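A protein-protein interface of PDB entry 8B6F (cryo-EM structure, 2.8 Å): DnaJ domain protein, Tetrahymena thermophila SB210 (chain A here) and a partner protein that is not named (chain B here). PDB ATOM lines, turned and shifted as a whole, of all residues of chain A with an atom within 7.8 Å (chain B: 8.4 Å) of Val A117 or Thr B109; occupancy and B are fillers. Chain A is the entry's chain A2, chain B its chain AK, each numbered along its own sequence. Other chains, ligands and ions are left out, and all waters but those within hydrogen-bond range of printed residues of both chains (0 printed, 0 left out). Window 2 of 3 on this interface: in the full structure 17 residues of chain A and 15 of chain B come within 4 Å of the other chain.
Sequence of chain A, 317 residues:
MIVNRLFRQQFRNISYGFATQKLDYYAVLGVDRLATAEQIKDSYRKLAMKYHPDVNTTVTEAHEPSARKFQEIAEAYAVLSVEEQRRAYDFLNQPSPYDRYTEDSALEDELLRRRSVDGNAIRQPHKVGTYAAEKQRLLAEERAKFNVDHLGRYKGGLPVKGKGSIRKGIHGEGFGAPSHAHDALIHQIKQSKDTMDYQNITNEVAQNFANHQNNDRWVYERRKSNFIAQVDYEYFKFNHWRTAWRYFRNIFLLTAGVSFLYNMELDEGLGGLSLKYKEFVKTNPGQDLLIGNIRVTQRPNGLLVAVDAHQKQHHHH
N of Leu A151 sits close to OD1 of Asp A149, 3.3 Å away.
The side-chain carboxylate (OD2) of Asp A118 lies within hydrogen-bond range of the side-chain amide nitrogen (ND2) of Asn A120 (2.8 Å).
The side-chain hydroxyl (OG1) of Thr B109 sits close to the side-chain amide nitrogen (NE2) of Gln B111, 3.2 Å away.
Of the 13 printed residues of chain B, 3 touch a printed residue of chain A.
Among the printed residues, no Asp or Glu carboxylate lies within 4 Å of a Lys or Arg side-chain nitrogen of the other chain.
Among the printed residues, merely in contact across the chains: Val A117 with Thr B109, Asp A118 with Pro B108, Asp A118 with Thr B109, Asp A149 with Gly B110 and His A150 with Pro B108.
Of the printed residues of chain A, Thr B109 touches Val A117 (3.6 Å) and Asp A118 (3.3 Å).
No residue of chain B comes within 4 Å of Ser A116.
Pro B108 touches just these residues of chain A: Asp A118 (3.2 Å) and His A150 (3.2 Å).
Printed residues of chain B within 4 Å of His A150: Pro B108 (3.2 Å).
Of the printed residues of chain A, Gly B110 touches Asp A149 (3.9 Å).
Ser B106 touches none of the printed residues of chain A.
Arg A115 touches none of the printed residues of chain B.
The nearest residue of chain A that does not touch Thr B109 is Leu A151 (4.03 Å).
The nearest printed residue of chain B that does not touch His A150 is Gly B110 (4.2 Å).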
ATOM      1  N   ARG A 115      27.797 -31.191 -11.659  1.00  0.00           N
ATOM      2  CA  ARG A 115      27.294 -30.129 -10.801  1.00  0.00           C
ATOM      3  C   ARG A 115      25.773 -30.071 -10.852  1.00  0.00           C
ATOM      4  O   ARG A 115      25.140 -30.525 -11.807  1.00  0.00           O
ATOM      5  CB  ARG A 115      27.872 -28.769 -11.210  1.00  0.00           C
ATOM      6  CG  ARG A 115      29.365 -28.637 -10.983  1.00  0.00           C
ATOM      7  CD  ARG A 115      29.871 -27.298 -11.484  1.00  0.00           C
ATOM      8  NE  ARG A 115      31.221 -27.013 -11.016  1.00  0.00           N
ATOM      9  CZ  ARG A 115      31.858 -25.868 -11.221  1.00  0.00           C
ATOM     10  NH1 ARG A 115      31.294 -24.873 -11.885  1.00  0.00           N
ATOM     11  NH2 ARG A 115      33.088 -25.716 -10.743  1.00  0.00           N
ATOM     12  N   SER A 116      25.192 -29.496  -9.799  1.00  0.00           N
ATOM     13  CA  SER A 116      23.750 -29.328  -9.696  1.00  0.00           C
ATOM     14  C   SER A 116      23.333 -28.032 -10.388  1.00  0.00           C
ATOM     15  O   SER A 116      24.127 -27.381 -11.070  1.00  0.00           O
ATOM     16  CB  SER A 116      23.319 -29.329  -8.232  1.00  0.00           C
ATOM     17  OG  SER A 116      23.784 -30.481  -7.557  1.00  0.00           O
ATOM     18  N   VAL A 117      22.071 -27.641 -10.213  1.00  0.00           N
ATOM     19  CA  VAL A 117      21.593 -26.399 -10.813  1.00  0.00           C
ATOM     20  C   VAL A 117      22.278 -25.199 -10.172  1.00  0.00           C
ATOM     21  O   VAL A 117      22.565 -24.201 -10.841  1.00  0.00           O
ATOM     22  CB  VAL A 117      20.061 -26.307 -10.699  1.00  0.00           C
ATOM     23  CG1 VAL A 117      19.553 -25.009 -11.310  1.00  0.00           C
ATOM     24  CG2 VAL A 117      19.407 -27.503 -11.370  1.00  0.00           C
ATOM     25  N   ASP A 118      22.544 -25.271  -8.868  1.00  0.00           N
ATOM     26  CA  ASP A 118      23.197 -24.169  -8.173  1.00  0.00           C
ATOM     27  C   ASP A 118      24.684 -24.077  -8.481  1.00  0.00           C
ATOM     28  O   ASP A 118      25.317 -23.090  -8.094  1.00  0.00           O
ATOM     29  CB  ASP A 118      22.991 -24.304  -6.662  1.00  0.00           C
ATOM     30  CG  ASP A 118      23.543 -25.600  -6.109  1.00  0.00           C
ATOM     31  OD1 ASP A 118      24.127 -26.380  -6.889  1.00  0.00           O
ATOM     32  OD2 ASP A 118      23.392 -25.841  -4.895  1.00  0.00           O
ATOM     33  N   GLY A 119      25.256 -25.069  -9.161  1.00  0.00           N
ATOM     34  CA  GLY A 119      26.663 -25.071  -9.492  1.00  0.00           C
ATOM     35  C   GLY A 119      27.535 -25.857  -8.540  1.00  0.00           C
ATOM     36  O   GLY A 119      28.694 -26.126  -8.869  1.00  0.00           O
ATOM     37  N   ASN A 120      27.022 -26.219  -7.370  1.00  0.00           N
ATOM     38  CA  ASN A 120      27.784 -27.038  -6.442  1.00  0.00           C
ATOM     39  C   ASN A 120      27.858 -28.477  -6.938  1.00  0.00           C
ATOM     40  O   ASN A 120      26.922 -28.997  -7.549  1.00  0.00           O
ATOM     41  CB  ASN A 120      27.152 -26.993  -5.053  1.00  0.00           C
ATOM     42  CG  ASN A 120      27.075 -25.589  -4.494  1.00  0.00           C
ATOM     43  OD1 ASN A 120      28.017 -24.807  -4.614  1.00  0.00           O
ATOM     44  ND2 ASN A 120      25.944 -25.258  -3.885  1.00  0.00           N
ATOM     45  N   ILE A 122      27.864 -32.533  -6.992  1.00  0.00           N
ATOM     46  CA  ILE A 122      26.925 -33.482  -6.408  1.00  0.00           C
ATOM     47  C   ILE A 122      27.572 -34.157  -5.206  1.00  0.00           C
ATOM     48  O   ILE A 122      28.699 -34.661  -5.287  1.00  0.00           O
ATOM     49  CB  ILE A 122      26.481 -34.515  -7.454  1.00  0.00           C
ATOM     50  CG1 ILE A 122      25.743 -33.830  -8.611  1.00  0.00           C
ATOM     51  CG2 ILE A 122      25.613 -35.599  -6.811  1.00  0.00           C
ATOM     52  CD1 ILE A 122      24.359 -33.330  -8.263  1.00  0.00           C
ATOM     53  N   ASP A 149      20.850 -16.966   2.064  1.00  0.00           N
ATOM     54  CA  ASP A 149      20.827 -18.043   1.089  1.00  0.00           C
ATOM     55  C   ASP A 149      21.667 -19.218   1.584  1.00  0.00           C
ATOM     56  O   ASP A 149      22.290 -19.171   2.646  1.00  0.00           O
ATOM     57  CB  ASP A 149      21.313 -17.545  -0.271  1.00  0.00           C
ATOM     58  CG  ASP A 149      22.770 -17.124  -0.259  1.00  0.00           C
ATOM     59  OD1 ASP A 149      23.404 -17.178   0.815  1.00  0.00           O
ATOM     60  OD2 ASP A 149      23.283 -16.733  -1.329  1.00  0.00           O
ATOM     61  N   HIS A 150      21.688 -20.295   0.796  1.00  0.00           N
ATOM     62  CA  HIS A 150      22.358 -21.517   1.221  1.00  0.00           C
ATOM     63  C   HIS A 150      23.865 -21.344   1.366  1.00  0.00           C
ATOM     64  O   HIS A 150      24.497 -22.139   2.068  1.00  0.00           O
ATOM     65  CB  HIS A 150      22.058 -22.648   0.234  1.00  0.00           C
ATOM     66  CG  HIS A 150      22.549 -22.387  -1.155  1.00  0.00           C
ATOM     67  ND1 HIS A 150      21.897 -21.544  -2.030  1.00  0.00           N
ATOM     68  CD2 HIS A 150      23.623 -22.864  -1.825  1.00  0.00           C
ATOM     69  CE1 HIS A 150      22.553 -21.509  -3.176  1.00  0.00           C
ATOM     70  NE2 HIS A 150      23.605 -22.302  -3.078  1.00  0.00           N
ATOM     71  N   LEU A 151      24.453 -20.338   0.726  1.00  0.00           N
ATOM     72  CA  LEU A 151      25.885 -20.095   0.821  1.00  0.00           C
ATOM     73  C   LEU A 151      26.250 -19.106   1.919  1.00  0.00           C
ATOM     74  O   LEU A 151      27.429 -18.764   2.054  1.00  0.00           O
ATOM     75  CB  LEU A 151      26.428 -19.586  -0.520  1.00  0.00           C
ATOM     76  CG  LEU A 151      26.390 -20.557  -1.703  1.00  0.00           C
ATOM     77  CD1 LEU A 151      27.014 -19.913  -2.926  1.00  0.00           C
ATOM     78  CD2 LEU A 151      27.088 -21.868  -1.379  1.00  0.00           C
ATOM     79  N   SER B 106      16.356 -13.648  -5.771  1.00  0.00           N
ATOM     80  CA  SER B 106      17.614 -14.366  -5.636  1.00  0.00           C
ATOM     81  C   SER B 106      17.773 -15.297  -6.828  1.00  0.00           C
ATOM     82  O   SER B 106      16.841 -15.504  -7.609  1.00  0.00           O
ATOM     83  CB  SER B 106      17.670 -15.148  -4.322  1.00  0.00           C
ATOM     84  OG  SER B 106      16.656 -16.136  -4.274  1.00  0.00           O
ATOM     85  N   LEU B 107      18.974 -15.856  -6.960  1.00  0.00           N
ATOM     86  CA  LEU B 107      19.281 -16.836  -7.987  1.00  0.00           C
ATOM     87  C   LEU B 107      19.650 -18.170  -7.346  1.00  0.00           C
ATOM     88  O   LEU B 107      20.234 -18.197  -6.260  1.00  0.00           O
ATOM     89  CB  LEU B 107      20.438 -16.368  -8.879  1.00  0.00           C
ATOM     90  CG  LEU B 107      20.166 -15.154  -9.768  1.00  0.00           C
ATOM     91  CD1 LEU B 107      21.435 -14.726 -10.477  1.00  0.00           C
ATOM     92  CD2 LEU B 107      19.072 -15.451 -10.778  1.00  0.00           C
ATOM     93  N   PRO B 108      19.321 -19.293  -7.990  1.00  0.00           N
ATOM     94  CA  PRO B 108      19.678 -20.593  -7.399  1.00  0.00           C
ATOM     95  C   PRO B 108      21.171 -20.777  -7.211  1.00  0.00           C
ATOM     96  O   PRO B 108      21.589 -21.438  -6.252  1.00  0.00           O
ATOM     97  CB  PRO B 108      19.098 -21.605  -8.398  1.00  0.00           C
ATOM     98  CG  PRO B 108      18.968 -20.860  -9.674  1.00  0.00           C
ATOM     99  CD  PRO B 108      18.658 -19.445  -9.296  1.00  0.00           C
ATOM    100  N   THR B 109      21.992 -20.215  -8.097  1.00  0.00           N
ATOM    101  CA  THR B 109      23.436 -20.365  -7.994  1.00  0.00           C
ATOM    102  C   THR B 109      24.032 -19.571  -6.840  1.00  0.00           C
ATOM    103  O   THR B 109      25.210 -19.766  -6.522  1.00  0.00           O
ATOM    104  CB  THR B 109      24.104 -19.936  -9.303  1.00  0.00           C
ATOM    105  OG1 THR B 109      23.796 -18.564  -9.575  1.00  0.00           O
ATOM    106  CG2 THR B 109      23.620 -20.799 -10.457  1.00  0.00           C
ATOM    107  N   GLY B 110      23.259 -18.693  -6.207  1.00  0.00           N
ATOM    108  CA  GLY B 110      23.767 -17.850  -5.148  1.00  0.00           C
ATOM    109  C   GLY B 110      24.386 -16.552  -5.612  1.00  0.00           C
ATOM    110  O   GLY B 110      24.806 -15.750  -4.770  1.00  0.00           O
ATOM    111  N   GLN B 111      24.457 -16.319  -6.919  1.00  0.00           N
ATOM    112  CA  GLN B 111      25.013 -15.086  -7.437  1.00  0.00           C
ATOM    113  C   GLN B 111      24.092 -13.915  -7.115  1.00  0.00           C
ATOM    114  O   GLN B 111      22.904 -14.103  -6.850  1.00  0.00           O
ATOM    115  CB  GLN B 111      25.194 -15.184  -8.948  1.00  0.00           C
ATOM    116  CG  GLN B 111      26.025 -16.357  -9.395  1.00  0.00           C
ATOM    117  CD  GLN B 111      26.000 -16.535 -10.894  1.00  0.00           C
ATOM    118  OE1 GLN B 111      25.637 -15.623 -11.634  1.00  0.00           O
ATOM    119  NE2 GLN B 111      26.371 -17.721 -11.352  1.00  0.00           N
ATOM    120  N   PRO B 112      24.620 -12.692  -7.120  1.00  0.00           N
ATOM    121  CA  PRO B 112      23.744 -11.527  -6.957  1.00  0.00           C
ATOM    122  C   PRO B 112      22.676 -11.498  -8.040  1.00  0.00           C
ATOM    123  O   PRO B 112      22.941 -11.789  -9.207  1.00  0.00           O
ATOM    124  CB  PRO B 112      24.705 -10.338  -7.068  1.00  0.00           C
ATOM    125  CG  PRO B 112      25.941 -10.881  -7.692  1.00  0.00           C
ATOM    126  CD  PRO B 112      26.033 -12.300  -7.249  1.00  0.00           C
ATOM    127  N   ALA B 113      21.458 -11.140  -7.640  1.00  0.00           N
ATOM    128  CA  ALA B 113      20.312 -11.138  -8.539  1.00  0.00           C
ATOM    129  C   ALA B 113      20.038  -9.768  -9.142  1.00  0.00           C
ATOM    130  O   ALA B 113      18.964  -9.558  -9.711  1.00  0.00           O
ATOM    131  CB  ALA B 113      19.069 -11.638  -7.803  1.00  0.00           C
ATOM    132  N   GLU B 148      15.887 -15.032 -15.724  1.00  0.00           N
ATOM    133  CA  GLU B 148      16.800 -14.779 -14.616  1.00  0.00           C
ATOM    134  C   GLU B 148      18.015 -15.695 -14.673  1.00  0.00           C
ATOM    135  O   GLU B 148      17.905 -16.885 -14.980  1.00  0.00           O
ATOM    136  CB  GLU B 148      16.078 -14.960 -13.275  1.00  0.00           C
ATOM    137  CG  GLU B 148      15.713 -16.400 -12.914  1.00  0.00           C
ATOM    138  CD  GLU B 148      14.632 -16.983 -13.797  1.00  0.00           C
ATOM    139  OE1 GLU B 148      14.065 -16.237 -14.621  1.00  0.00           O
ATOM    140  OE2 GLU B 148      14.345 -18.192 -13.668  1.00  0.00           O
ATOM    141  N   GLY B 149      19.183 -15.132 -14.370  1.00  0.00           N
ATOM    142  CA  GLY B 149      20.416 -15.884 -14.335  1.00  0.00           C
ATOM    143  C   GLY B 149      21.167 -15.953 -15.646  1.00  0.00           C
ATOM    144  O   GLY B 149      22.290 -16.469 -15.668  1.00  0.00           O
ATOM    145  N   PRO B 166      16.633 -19.411 -18.225  1.00  0.00           N
ATOM    146  CA  PRO B 166      17.357 -18.996 -17.018  1.00  0.00           C
ATOM    147  C   PRO B 166      18.707 -19.687 -16.908  1.00  0.00           C
ATOM    148  O   PRO B 166      18.857 -20.860 -17.254  1.00  0.00           O
ATOM    149  CB  PRO B 166      16.421 -19.417 -15.879  1.00  0.00           C
ATOM    150  CG  PRO B 166      15.099 -19.672 -16.513  1.00  0.00           C
ATOM    151  CD  PRO B 166      15.401 -20.145 -17.893  1.00  0.00           C
ATOM    152  N   GLY B 167      19.691 -18.945 -16.413  1.00  0.00           N
ATOM    153  CA  GLY B 167      21.000 -19.524 -16.156  1.00  0.00           C
ATOM    154  C   GLY B 167      21.676 -20.089 -17.384  1.00  0.00           C
ATOM    155  O   GLY B 167      22.315 -21.145 -17.307  1.00  0.00           O
ATOM    156  N   ARG B 168      21.553 -19.407 -18.519  1.00  0.00           N
ATOM    157  CA  ARG B 168      22.196 -19.810 -19.761  1.00  0.00           C
ATOM    158  C   ARG B 168      23.255 -18.787 -20.141  1.00  0.00           C
ATOM    159  O   ARG B 168      23.056 -17.580 -19.972  1.00  0.00           O
ATOM    160  CB  ARG B 168      21.177 -19.950 -20.895  1.00  0.00           C
ATOM    161  CG  ARG B 168      20.254 -21.146 -20.759  1.00  0.00           C
ATOM    162  CD  ARG B 168      21.020 -22.451 -20.879  1.00  0.00           C
ATOM    163  NE  ARG B 168      20.134 -23.608 -20.846  1.00  0.00           N
ATOM    164  CZ  ARG B 168      19.660 -24.158 -19.736  1.00  0.00           C
ATOM    165  NH1 ARG B 168      19.949 -23.666 -18.542  1.00  0.00           N
ATOM    166  NH2 ARG B 168      18.876 -25.228 -19.826  1.00  0.00           N
